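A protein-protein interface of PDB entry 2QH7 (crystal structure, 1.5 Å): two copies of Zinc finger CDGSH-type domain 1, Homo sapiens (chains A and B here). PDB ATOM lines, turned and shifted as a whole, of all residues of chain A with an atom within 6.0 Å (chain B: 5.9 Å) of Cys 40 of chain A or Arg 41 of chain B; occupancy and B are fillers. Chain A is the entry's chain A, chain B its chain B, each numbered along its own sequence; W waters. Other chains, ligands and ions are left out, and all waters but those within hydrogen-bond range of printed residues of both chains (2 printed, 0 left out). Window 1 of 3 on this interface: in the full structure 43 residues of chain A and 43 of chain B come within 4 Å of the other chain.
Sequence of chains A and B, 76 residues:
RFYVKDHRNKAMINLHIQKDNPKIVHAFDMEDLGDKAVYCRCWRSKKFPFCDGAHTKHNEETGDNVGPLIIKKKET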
ATOM      1  N   ILE A  13      -9.160 -12.305  17.064  1.00  0.00           N
ATOM      2  CA  ILE A  13     -10.210 -12.346  18.073  1.00  0.00           C
ATOM      3  C   ILE A  13     -11.579 -12.048  17.455  1.00  0.00           C
ATOM      4  O   ILE A  13     -12.524 -12.802  17.653  1.00  0.00           O
ATOM      5  CB  ILE A  13      -9.868 -11.338  19.195  1.00  0.00           C
ATOM      6  CG1 ILE A  13      -8.671 -11.862  20.002  1.00  0.00           C
ATOM      7  CG2 ILE A  13     -11.043 -11.008  20.108  1.00  0.00           C
ATOM      8  CD1 ILE A  13      -8.132 -10.822  20.982  1.00  0.00           C
ATOM      9  N   ILE A  24     -11.956  -1.009  15.824  1.00  0.00           N
ATOM     10  CA  ILE A  24     -13.258  -0.831  16.412  1.00  0.00           C
ATOM     11  C   ILE A  24     -13.139  -0.373  17.865  1.00  0.00           C
ATOM     12  O   ILE A  24     -12.728  -1.125  18.729  1.00  0.00           O
ATOM     13  CB  ILE A  24     -14.133  -2.091  16.293  1.00  0.00           C
ATOM     14  CG1 ILE A  24     -14.331  -2.477  14.820  1.00  0.00           C
ATOM     15  CG2 ILE A  24     -15.504  -1.846  17.014  1.00  0.00           C
ATOM     16  CD1 ILE A  24     -14.839  -3.871  14.630  1.00  0.00           C
ATOM     17  N   VAL A  25     -13.552   0.877  18.094  1.00  0.00           N
ATOM     18  CA  VAL A  25     -13.543   1.536  19.394  1.00  0.00           C
ATOM     19  C   VAL A  25     -14.952   2.068  19.616  1.00  0.00           C
ATOM     20  O   VAL A  25     -15.606   2.586  18.698  1.00  0.00           O
ATOM     21  CB  VAL A  25     -12.536   2.722  19.429  1.00  0.00           C
ATOM     22  CG1 VAL A  25     -12.534   3.444  20.809  1.00  0.00           C
ATOM     23  CG2 VAL A  25     -11.116   2.286  19.036  1.00  0.00           C
ATOM     24  N   HIS A  26     -15.433   1.939  20.846  1.00  0.00           N
ATOM     25  CA  HIS A  26     -16.702   2.568  21.242  1.00  0.00           C
ATOM     26  C   HIS A  26     -16.493   3.507  22.399  1.00  0.00           C
ATOM     27  O   HIS A  26     -15.669   3.254  23.283  1.00  0.00           O
ATOM     28  CB  HIS A  26     -17.753   1.516  21.601  1.00  0.00           C
ATOM     29  CG  HIS A  26     -18.269   0.760  20.412  1.00  0.00           C
ATOM     30  ND1 HIS A  26     -17.637  -0.349  19.889  1.00  0.00           N
ATOM     31  CD2 HIS A  26     -19.343   0.973  19.622  1.00  0.00           C
ATOM     32  CE1 HIS A  26     -18.302  -0.789  18.837  1.00  0.00           C
ATOM     33  NE2 HIS A  26     -19.352  -0.011  18.663  1.00  0.00           N
ATOM     34  N   VAL A  38     -24.310  -3.671  29.524  1.00  0.00           N
ATOM     35  CA  VAL A  38     -23.550  -4.891  29.546  1.00  0.00           C
ATOM     36  C   VAL A  38     -22.864  -4.991  28.213  1.00  0.00           C
ATOM     37  O   VAL A  38     -23.518  -5.197  27.201  1.00  0.00           O
ATOM     38  CB  VAL A  38     -24.458  -6.117  29.782  1.00  0.00           C
ATOM     39  CG1 VAL A  38     -23.597  -7.393  29.940  1.00  0.00           C
ATOM     40  CG2 VAL A  38     -25.251  -5.918  31.006  1.00  0.00           C
ATOM     41  N   TYR A  39     -21.529  -4.887  28.221  1.00  0.00           N
ATOM     42  CA  TYR A  39     -20.758  -4.717  27.004  1.00  0.00           C
ATOM     43  C   TYR A  39     -20.025  -5.989  26.664  1.00  0.00           C
ATOM     44  O   TYR A  39     -19.451  -6.637  27.524  1.00  0.00           O
ATOM     45  CB  TYR A  39     -19.762  -3.591  27.177  1.00  0.00           C
ATOM     46  CG  TYR A  39     -20.408  -2.244  27.358  1.00  0.00           C
ATOM     47  CD1 TYR A  39     -21.012  -1.599  26.285  1.00  0.00           C
ATOM     48  CD2 TYR A  39     -20.378  -1.592  28.591  1.00  0.00           C
ATOM     49  CE1 TYR A  39     -21.580  -0.373  26.427  1.00  0.00           C
ATOM     50  CE2 TYR A  39     -20.946  -0.349  28.748  1.00  0.00           C
ATOM     51  CZ  TYR A  39     -21.557   0.251  27.658  1.00  0.00           C
ATOM     52  OH  TYR A  39     -22.118   1.478  27.815  1.00  0.00           O
ATOM     53  N   CYS A  40     -20.020  -6.329  25.388  1.00  0.00           N
ATOM     54  CA  CYS A  40     -19.403  -7.538  24.925  1.00  0.00           C
ATOM     55  C   CYS A  40     -17.858  -7.459  24.853  1.00  0.00           C
ATOM     56  O   CYS A  40     -17.286  -6.500  24.326  1.00  0.00           O
ATOM     57  CB  CYS A  40     -20.001  -7.864  23.550  1.00  0.00           C
ATOM     58  SG  CYS A  40     -19.228  -9.278  22.734  1.00  0.00           S
ATOM     59  N   ARG A  41     -17.166  -8.456  25.386  1.00  0.00           N
ATOM     60  CA  ARG A  41     -15.711  -8.507  25.274  1.00  0.00           C
ATOM     61  C   ARG A  41     -15.230  -9.720  24.497  1.00  0.00           C
ATOM     62  O   ARG A  41     -14.077 -10.077  24.471  1.00  0.00           O
ATOM     63  CB  ARG A  41     -15.038  -8.449  26.658  1.00  0.00           C
ATOM     64  CG  ARG A  41     -15.361  -7.184  27.417  1.00  0.00           C
ATOM     65  CD  ARG A  41     -14.511  -7.060  28.665  1.00  0.00           C
ATOM     66  NE  ARG A  41     -14.787  -8.084  29.681  1.00  0.00           N
ATOM     67  CZ  ARG A  41     -14.309  -8.078  30.929  1.00  0.00           C
ATOM     68  NH1 ARG A  41     -13.547  -7.090  31.391  1.00  0.00           N
ATOM     69  NH2 ARG A  41     -14.638  -9.061  31.765  1.00  0.00           N
ATOM     70  N   CYS A  42     -16.163 -10.399  23.855  1.00  0.00           N
ATOM     71  CA  CYS A  42     -15.842 -11.603  23.100  1.00  0.00           C
ATOM     72  C   CYS A  42     -15.954 -11.431  21.590  1.00  0.00           C
ATOM     73  O   CYS A  42     -15.596 -12.341  20.863  1.00  0.00           O
ATOM     74  CB  CYS A  42     -16.746 -12.780  23.535  1.00  0.00           C
ATOM     75  SG  CYS A  42     -18.514 -12.689  23.060  1.00  0.00           S
ATOM     76  N   TRP A  43     -16.516 -10.330  21.104  1.00  0.00           N
ATOM     77  CA  TRP A  43     -16.682 -10.128  19.643  1.00  0.00           C
ATOM     78  C   TRP A  43     -17.530 -11.191  18.938  1.00  0.00           C
ATOM     79  O   TRP A  43     -17.343 -11.467  17.770  1.00  0.00           O
ATOM     80  CB  TRP A  43     -15.302  -9.936  18.975  1.00  0.00           C
ATOM     81  CG  TRP A  43     -14.556  -8.845  19.627  1.00  0.00           C
ATOM     82  CD1 TRP A  43     -13.801  -8.938  20.748  1.00  0.00           C
ATOM     83  CD2 TRP A  43     -14.493  -7.477  19.216  1.00  0.00           C
ATOM     84  NE1 TRP A  43     -13.300  -7.719  21.086  1.00  0.00           N
ATOM     85  CE2 TRP A  43     -13.686  -6.806  20.156  1.00  0.00           C
ATOM     86  CE3 TRP A  43     -15.015  -6.761  18.128  1.00  0.00           C
ATOM     87  CZ2 TRP A  43     -13.413  -5.456  20.068  1.00  0.00           C
ATOM     88  CZ3 TRP A  43     -14.734  -5.416  18.038  1.00  0.00           C
ATOM     89  CH2 TRP A  43     -13.939  -4.778  18.984  1.00  0.00           C
ATOM     90  N   ARG A  44     -18.507 -11.750  19.652  1.00  0.00           N
ATOM     91  CA  ARG A  44     -19.439 -12.706  19.073  1.00  0.00           C
ATOM     92  C   ARG A  44     -20.883 -12.261  19.174  1.00  0.00           C
ATOM     93  O   ARG A  44     -21.749 -12.917  18.595  1.00  0.00           O
ATOM     94  CB  ARG A  44     -19.295 -14.094  19.719  1.00  0.00           C
ATOM     95  CG  ARG A  44     -17.899 -14.739  19.600  1.00  0.00           C
ATOM     96  CD  ARG A  44     -17.543 -15.122  18.180  1.00  0.00           C
ATOM     97  NE  ARG A  44     -16.208 -15.713  18.128  1.00  0.00           N
ATOM     98  CZ  ARG A  44     -15.079 -15.017  17.998  1.00  0.00           C
ATOM     99  NH1 ARG A  44     -15.111 -13.712  17.809  1.00  0.00           N
ATOM    100  NH2 ARG A  44     -13.914 -15.649  17.980  1.00  0.00           N
ATOM    101  N   SER A  45     -21.167 -11.172  19.886  1.00  0.00           N
ATOM    102  CA  SER A  45     -22.544 -10.739  20.068  1.00  0.00           C
ATOM    103  C   SER A  45     -23.120 -10.195  18.775  1.00  0.00           C
ATOM    104  O   SER A  45     -22.435  -9.516  18.034  1.00  0.00           O
ATOM    105  CB  SER A  45     -22.621  -9.631  21.096  1.00  0.00           C
ATOM    106  OG  SER A  45     -23.968  -9.210  21.256  1.00  0.00           O
ATOM    107  N   PHE A  48     -23.386  -6.362  19.222  1.00  0.00           N
ATOM    108  CA  PHE A  48     -22.124  -5.680  19.520  1.00  0.00           C
ATOM    109  C   PHE A  48     -22.271  -4.151  19.289  1.00  0.00           C
ATOM    110  O   PHE A  48     -22.820  -3.730  18.282  1.00  0.00           O
ATOM    111  CB  PHE A  48     -20.949  -6.271  18.713  1.00  0.00           C
ATOM    112  CG  PHE A  48     -19.587  -5.893  19.256  1.00  0.00           C
ATOM    113  CD1 PHE A  48     -18.957  -4.726  18.855  1.00  0.00           C
ATOM    114  CD2 PHE A  48     -18.952  -6.667  20.231  1.00  0.00           C
ATOM    115  CE1 PHE A  48     -17.742  -4.365  19.399  1.00  0.00           C
ATOM    116  CE2 PHE A  48     -17.712  -6.318  20.746  1.00  0.00           C
ATOM    117  CZ  PHE A  48     -17.128  -5.160  20.357  1.00  0.00           C
ATOM    118  N   PRO A  49     -21.791  -3.307  20.225  1.00  0.00           N
ATOM    119  CA  PRO A  49     -20.932  -3.498  21.392  1.00  0.00           C
ATOM    120  C   PRO A  49     -21.598  -4.102  22.655  1.00  0.00           C
ATOM    121  O   PRO A  49     -20.903  -4.326  23.651  1.00  0.00           O
ATOM    122  CB  PRO A  49     -20.496  -2.073  21.668  1.00  0.00           C
ATOM    123  CG  PRO A  49     -21.754  -1.310  21.364  1.00  0.00           C
ATOM    124  CD  PRO A  49     -22.149  -1.889  20.074  1.00  0.00           C
ATOM    125  N   PHE A  50     -22.899  -4.352  22.627  1.00  0.00           N
ATOM    126  CA  PHE A  50     -23.583  -4.932  23.769  1.00  0.00           C
ATOM    127  C   PHE A  50     -23.529  -6.451  23.776  1.00  0.00           C
ATOM    128  O   PHE A  50     -23.568  -7.104  22.730  1.00  0.00           O
ATOM    129  CB  PHE A  50     -25.009  -4.401  23.844  1.00  0.00           C
ATOM    130  CG  PHE A  50     -25.062  -2.910  23.911  1.00  0.00           C
ATOM    131  CD1 PHE A  50     -24.757  -2.249  25.093  1.00  0.00           C
ATOM    132  CD2 PHE A  50     -25.330  -2.165  22.774  1.00  0.00           C
ATOM    133  CE1 PHE A  50     -24.748  -0.867  25.147  1.00  0.00           C
ATOM    134  CE2 PHE A  50     -25.331  -0.777  22.824  1.00  0.00           C
ATOM    135  CZ  PHE A  50     -25.033  -0.133  24.009  1.00  0.00           C
ATOM    136  N   CYS A  51     -23.442  -6.996  24.985  1.00  0.00           N
ATOM    137  CA  CYS A  51     -23.456  -8.436  25.229  1.00  0.00           C
ATOM    138  C   CYS A  51     -24.860  -9.049  25.064  1.00  0.00           C
ATOM    139  O   CYS A  51     -25.866  -8.522  25.569  1.00  0.00           O
ATOM    140  CB  CYS A  51     -22.944  -8.688  26.654  1.00  0.00           C
ATOM    141  SG  CYS A  51     -23.010 -10.387  27.250  1.00  0.00           S
ATOM    142  N   ASP A  52     -24.924 -10.147  24.323  1.00  0.00           N
ATOM    143  CA  ASP A  52     -26.172 -10.891  24.122  1.00  0.00           C
ATOM    144  C   ASP A  52     -26.077 -12.355  24.577  1.00  0.00           C
ATOM    145  O   ASP A  52     -26.930 -13.173  24.205  1.00  0.00           O
ATOM    146  CB  ASP A  52     -26.651 -10.816  22.653  1.00  0.00           C
ATOM    147  CG  ASP A  52     -25.794 -11.656  21.683  1.00  0.00           C
ATOM    148  OD1 ASP A  52     -24.753 -12.223  22.115  1.00  0.00           O
ATOM    149  OD2 ASP A  52     -26.150 -11.716  20.487  1.00  0.00           O
ATOM    150  N   GLY A  67     -15.964 -13.087  29.402  1.00  0.00           N
ATOM    151  CA  GLY A  67     -17.305 -12.609  29.687  1.00  0.00           C
ATOM    152  C   GLY A  67     -17.344 -11.097  29.563  1.00  0.00           C
ATOM    153  O   GLY A  67     -16.308 -10.483  29.267  1.00  0.00           O
ATOM    154  N   PRO A  68     -18.508 -10.492  29.774  1.00  0.00           N
ATOM    155  CA  PRO A  68     -18.708  -9.059  29.573  1.00  0.00           C
ATOM    156  C   PRO A  68     -18.176  -8.079  30.643  1.00  0.00           C
ATOM    157  O   PRO A  68     -17.722  -8.467  31.726  1.00  0.00           O
ATOM    158  CB  PRO A  68     -20.241  -8.951  29.464  1.00  0.00           C
ATOM    159  CG  PRO A  68     -20.731 -10.033  30.363  1.00  0.00           C
ATOM    160  CD  PRO A  68     -19.769 -11.172  30.137  1.00  0.00           C
ATOM    161  N   LEU A  69     -18.231  -6.808  30.271  1.00  0.00           N
ATOM    162  CA  LEU A  69     -18.016  -5.663  31.138  1.00  0.00           C
ATOM    163  C   LEU A  69     -19.355  -4.982  31.420  1.00  0.00           C
ATOM    164  O   LEU A  69     -20.070  -4.576  30.504  1.00  0.00           O
ATOM    165  CB  LEU A  69     -17.113  -4.677  30.432  1.00  0.00           C
ATOM    166  CG  LEU A  69     -16.797  -3.434  31.246  1.00  0.00           C
ATOM    167  CD1 LEU A  69     -15.687  -3.728  32.240  1.00  0.00           C
ATOM    168  CD2 LEU A  69     -16.428  -2.339  30.330  1.00  0.00           C
ATOM    169  N   ILE B  13      -9.888 -16.675  22.823  1.00  0.00           N
ATOM    170  CA  ILE B  13      -9.642 -15.244  22.781  1.00  0.00           C
ATOM    171  C   ILE B  13      -8.683 -14.849  23.904  1.00  0.00           C
ATOM    172  O   ILE B  13      -7.649 -14.231  23.655  1.00  0.00           O
ATOM    173  CB  ILE B  13     -10.977 -14.478  22.880  1.00  0.00           C
ATOM    174  CG1 ILE B  13     -11.805 -14.731  21.614  1.00  0.00           C
ATOM    175  CG2 ILE B  13     -10.749 -12.998  23.096  1.00  0.00           C
ATOM    176  CD1 ILE B  13     -13.266 -14.313  21.729  1.00  0.00           C
ATOM    177  N   TYR B  39     -11.524   0.542  28.728  1.00  0.00           N
ATOM    178  CA  TYR B  39     -11.554  -0.898  28.993  1.00  0.00           C
ATOM    179  C   TYR B  39     -11.043  -1.720  27.813  1.00  0.00           C
ATOM    180  O   TYR B  39     -11.429  -1.480  26.648  1.00  0.00           O
ATOM    181  CB  TYR B  39     -12.958  -1.318  29.426  1.00  0.00           C
ATOM    182  CG  TYR B  39     -13.449  -0.613  30.669  1.00  0.00           C
ATOM    183  CD1 TYR B  39     -13.000  -0.982  31.947  1.00  0.00           C
ATOM    184  CD2 TYR B  39     -14.362   0.422  30.574  1.00  0.00           C
ATOM    185  CE1 TYR B  39     -13.475  -0.338  33.071  1.00  0.00           C
ATOM    186  CE2 TYR B  39     -14.840   1.058  31.684  1.00  0.00           C
ATOM    187  CZ  TYR B  39     -14.385   0.678  32.935  1.00  0.00           C
ATOM    188  OH  TYR B  39     -14.840   1.348  34.040  1.00  0.00           O
ATOM    189  N   CYS B  40     -10.251  -2.724  28.145  1.00  0.00           N
ATOM    190  CA  CYS B  40      -9.704  -3.644  27.178  1.00  0.00           C
ATOM    191  C   CYS B  40     -10.743  -4.622  26.642  1.00  0.00           C
ATOM    192  O   CYS B  40     -11.443  -5.300  27.378  1.00  0.00           O
ATOM    193  CB  CYS B  40      -8.545  -4.396  27.815  1.00  0.00           C
ATOM    194  SG  CYS B  40      -7.776  -5.641  26.757  1.00  0.00           S
ATOM    195  N   ARG B  41     -10.731  -4.837  25.342  1.00  0.00           N
ATOM    196  CA  ARG B  41     -11.675  -5.816  24.724  1.00  0.00           C
ATOM    197  C   ARG B  41     -10.883  -6.861  23.956  1.00  0.00           C
ATOM    198  O   ARG B  41     -11.442  -7.647  23.225  1.00  0.00           O
ATOM    199  CB  ARG B  41     -12.666  -5.112  23.804  1.00  0.00           C
ATOM    200  CG  ARG B  41     -13.704  -4.253  24.565  1.00  0.00           C
ATOM    201  CD  ARG B  41     -14.882  -3.723  23.848  1.00  0.00           C
ATOM    202  NE  ARG B  41     -14.509  -2.884  22.669  1.00  0.00           N
ATOM    203  CZ  ARG B  41     -15.424  -2.253  21.897  1.00  0.00           C
ATOM    204  NH1 ARG B  41     -16.729  -2.246  22.124  1.00  0.00           N
ATOM    205  NH2 ARG B  41     -14.974  -1.566  20.863  1.00  0.00           N
ATOM    206  N   CYS B  42      -9.543  -6.803  24.074  1.00  0.00           N
ATOM    207  CA  CYS B  42      -8.631  -7.707  23.359  1.00  0.00           C
ATOM    208  C   CYS B  42      -8.023  -8.757  24.247  1.00  0.00           C
ATOM    209  O   CYS B  42      -7.376  -9.640  23.752  1.00  0.00           O
ATOM    210  CB  CYS B  42      -7.482  -6.946  22.631  1.00  0.00           C
ATOM    211  SG  CYS B  42      -6.180  -6.257  23.663  1.00  0.00           S
ATOM    212  N   TRP B  43      -8.147  -8.651  25.557  1.00  0.00           N
ATOM    213  CA  TRP B  43      -7.518  -9.629  26.474  1.00  0.00           C
ATOM    214  C   TRP B  43      -5.998  -9.767  26.410  1.00  0.00           C
ATOM    215  O   TRP B  43      -5.429 -10.817  26.763  1.00  0.00           O
ATOM    216  CB  TRP B  43      -8.224 -10.988  26.305  1.00  0.00           C
ATOM    217  CG  TRP B  43      -9.713 -10.858  26.526  1.00  0.00           C
ATOM    218  CD1 TRP B  43     -10.610 -10.457  25.623  1.00  0.00           C
ATOM    219  CD2 TRP B  43     -10.441 -11.112  27.741  1.00  0.00           C
ATOM    220  NE1 TRP B  43     -11.862 -10.464  26.168  1.00  0.00           N
ATOM    221  CE2 TRP B  43     -11.788 -10.857  27.470  1.00  0.00           C
ATOM    222  CE3 TRP B  43     -10.073 -11.548  29.026  1.00  0.00           C
ATOM    223  CZ2 TRP B  43     -12.791 -10.988  28.436  1.00  0.00           C
ATOM    224  CZ3 TRP B  43     -11.070 -11.707  29.979  1.00  0.00           C
ATOM    225  CH2 TRP B  43     -12.413 -11.430  29.679  1.00  0.00           C
ATOM    226  N   PHE B  48      -5.360  -5.469  32.517  1.00  0.00           N
ATOM    227  CA  PHE B  48      -6.715  -5.923  32.331  1.00  0.00           C
ATOM    228  C   PHE B  48      -7.477  -5.832  33.653  1.00  0.00           C
ATOM    229  O   PHE B  48      -6.952  -6.228  34.687  1.00  0.00           O
ATOM    230  CB  PHE B  48      -6.747  -7.360  31.786  1.00  0.00           C
ATOM    231  CG  PHE B  48      -8.068  -7.737  31.221  1.00  0.00           C
ATOM    232  CD1 PHE B  48      -9.048  -8.345  32.009  1.00  0.00           C
ATOM    233  CD2 PHE B  48      -8.372  -7.430  29.895  1.00  0.00           C
ATOM    234  CE1 PHE B  48     -10.290  -8.656  31.481  1.00  0.00           C
ATOM    235  CE2 PHE B  48      -9.610  -7.737  29.358  1.00  0.00           C
ATOM    236  CZ  PHE B  48     -10.578  -8.337  30.146  1.00  0.00           C
ATOM    237  N   PRO B  49      -8.728  -5.325  33.634  1.00  0.00           N
ATOM    238  CA  PRO B  49      -9.695  -5.006  32.559  1.00  0.00           C
ATOM    239  C   PRO B  49      -9.450  -3.679  31.815  1.00  0.00           C
ATOM    240  O   PRO B  49     -10.233  -3.293  30.966  1.00  0.00           O
ATOM    241  CB  PRO B  49     -11.022  -4.955  33.319  1.00  0.00           C
ATOM    242  CG  PRO B  49     -10.633  -4.420  34.657  1.00  0.00           C
ATOM    243  CD  PRO B  49      -9.267  -4.974  34.961  1.00  0.00           C
ATOM    244  N   VAL B  66      -9.565  -4.895  16.475  1.00  0.00           N
ATOM    245  CA  VAL B  66     -10.216  -4.715  17.764  1.00  0.00           C
ATOM    246  C   VAL B  66      -9.663  -3.528  18.506  1.00  0.00           C
ATOM    247  O   VAL B  66      -8.565  -3.098  18.279  1.00  0.00           O
ATOM    248  CB  VAL B  66     -10.207  -6.007  18.673  1.00  0.00           C
ATOM    249  CG1 VAL B  66     -11.052  -7.117  18.002  1.00  0.00           C
ATOM    250  CG2 VAL B  66      -8.793  -6.467  19.029  1.00  0.00           C
ATOM    251  N   GLY B  67     -10.463  -2.984  19.385  1.00  0.00           N
ATOM    252  CA  GLY B  67     -10.089  -1.811  20.144  1.00  0.00           C
ATOM    253  C   GLY B  67     -10.888  -1.717  21.406  1.00  0.00           C
ATOM    254  O   GLY B  67     -11.827  -2.490  21.578  1.00  0.00           O
ATOM    255  N   PRO B  68     -10.545  -0.748  22.275  1.00  0.00           N
ATOM    256  CA  PRO B  68     -11.231  -0.532  23.564  1.00  0.00           C
ATOM    257  C   PRO B  68     -12.646   0.056  23.583  1.00  0.00           C
ATOM    258  O   PRO B  68     -13.217   0.453  22.575  1.00  0.00           O
ATOM    259  CB  PRO B  68     -10.246   0.383  24.316  1.00  0.00           C
ATOM    260  CG  PRO B  68      -9.580   1.151  23.241  1.00  0.00           C
ATOM    261  CD  PRO B  68      -9.390   0.152  22.118  1.00  0.00           C
ATOM    262  N   LEU B  69     -13.227  -0.048  24.770  1.00  0.00           N
ATOM    263  CA  LEU B  69     -14.454   0.600  25.148  1.00  0.00           C
ATOM    264  C   LEU B  69     -14.151   1.728  26.138  1.00  0.00           C
ATOM    265  O   LEU B  69     -13.566   1.546  27.227  1.00  0.00           O
ATOM    266  CB  LEU B  69     -15.382  -0.412  25.802  1.00  0.00           C
ATOM    267  CG  LEU B  69     -16.688   0.156  26.368  1.00  0.00           C
ATOM    268  CD1 LEU B  69     -17.694   0.507  25.286  1.00  0.00           C
ATOM    269  CD2 LEU B  69     -17.294  -0.811  27.327  1.00  0.00           C
HETATM  270  O   HOH W   1     -12.489  -4.906  29.988  1.00  0.00           O
HETATM  271  O   HOH W   2     -18.231  -3.878  23.891  1.00  0.00           O
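The backbone carbonyl oxygen (O) of Arg 41 of chain A is in hydrogen-bond range of the indole nitrogen (NE1) of Trp 43 of chain B (2.8 Å). O of Ile 24 of chain A lies within hydrogen-bond range of N of Gly 67 of chain B (3.0 Å). NE1 of Trp 43 of chain A lies within hydrogen-bond range of O of Arg 41 of chain B, 2.8 Å away. O of Ile 24 of chain A sits at hydrogen-bond distance from NH2 of Arg 41 of chain B, 3.1 Å away. ND1 of His 26 of chain A lies within hydrogen-bond range of NH1 of Arg 41 of chain B (3.1 Å). The backbone NH of His 26 of chain A lies within hydrogen-bond range of the backbone carbonyl oxygen of Pro 68 of chain B.
The backbone carbonyl oxygen (O) of Ile 13 of chain A sits at hydrogen-bond distance from the guanidinium group (NH1) of Arg 44 of chain A (2.7 Å). The guanidinium group (NH2) of Arg 41 of chain B lies within hydrogen-bond range of the backbone carbonyl oxygen (O) of Pro 68 of chain B (3.2 Å). The guanidinium group (NH2) of Arg 41 of chain A sits at hydrogen-bond distance from the backbone carbonyl oxygen (O) of Pro 68 of chain A, 3.1 Å away. The backbone NH of Tyr 39 of chain A sits at hydrogen-bond distance from the backbone carbonyl oxygen of Leu 69 of chain A. The backbone carbonyl oxygen of Pro 49 of chain B lies within hydrogen-bond range of the backbone NH of Cys 40 of chain B (2.9 Å). The side-chain sulfur (SG) of Cys 40 of chain A sits close to the backbone NH (N) of Trp 43 of chain A.
CD1 of Ile 13 of chain A touches O of Cys 42 of chain B (3.1 Å). O of Ile 24 of chain A touches C of Val 66 of chain B, at 3.9 Å. Val 25 of chain A touches Arg 41 of chain B (CA to NH2, 3.7 Å). Val 25 of chain A touches Pro 68 of chain B (CA to O, 3.4 Å). CA of Leu 69 of chain B touches O of His 26 of chain A, at 3.5 Å. Tyr 39 of chain A touches Leu 69 of chain B. Arg 41 of chain A touches Cys 40 of chain B. Trp 43 of chain B touches Gly 67 of chain A (CZ2 to O, 3.6 Å). Leu 69 of chain A touches Tyr 39 of chain B (CD2 to CD2, 3.5 Å). Leu 69 of chain A touches Leu 69 of chain B.
Of chain B, only Arg 41 (3.7 Å) comes within 4 Å of Cys 40 of chain A. Of chain A, only Ile 24 (3.1 Å), Val 25 (3.7 Å), His 26 (3.1 Å), Cys 40 (3.7 Å), Arg 41 (3.8 Å), Trp 43 (2.8 Å), Phe 48 (3.4 Å) and Pro 49 (3.8 Å) come within 4 Å of Arg 41 of chain B. Of the printed residues of chain B, Trp 43 of chain A touches Arg 41 (2.8 Å), Val 66 (3.4 Å) and Gly 67 (3.7 Å). Of the printed residues of chain B, Phe 48 of chain A touches Arg 41 (3.4 Å). Of the printed residues of chain A, Ile 13 of chain B touches Ile 13 and Cys 42. The nearest printed residue of chain A that does not touch Pro 49 of chain B is Leu 69 of chain A (4.9 Å).
Of the 12 printed residues of chain B, 12 touch a printed residue of chain A. Hydrophobic or aromatic side chains of chain B that line the printed part of chain A: Ile 13, Tyr 39, Trp 43, Phe 48, Pro 49, Val 66 and Leu 69. Along chain B the printed residues that touch a printed residue of chain A span positions 13 to 69.
Ile 13 of chain A touches its own counterpart, Ile 13 of chain B. Tyr 39 of chain A touches Leu 69 of chain B, and with the chains exchanged Leu 69 of chain A touches Tyr 39 of chain B. Cys 40 of chain A touches Arg 41 of chain B, and with the chains exchanged Arg 41 of chain A touches Cys 40 of chain B. Arg 41 of chain A touches its own counterpart, Arg 41 of chain B.
Water W2 lies within hydrogen-bond range of O of Pro 49 of chain A, O of Cys 40 of chain A and NH1 of Arg 41 of chain B. Water W1 lies within hydrogen-bond range of NH1 of Arg 41 of chain A, O of Cys 40 of chain B and O of Pro 49 of chain B.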
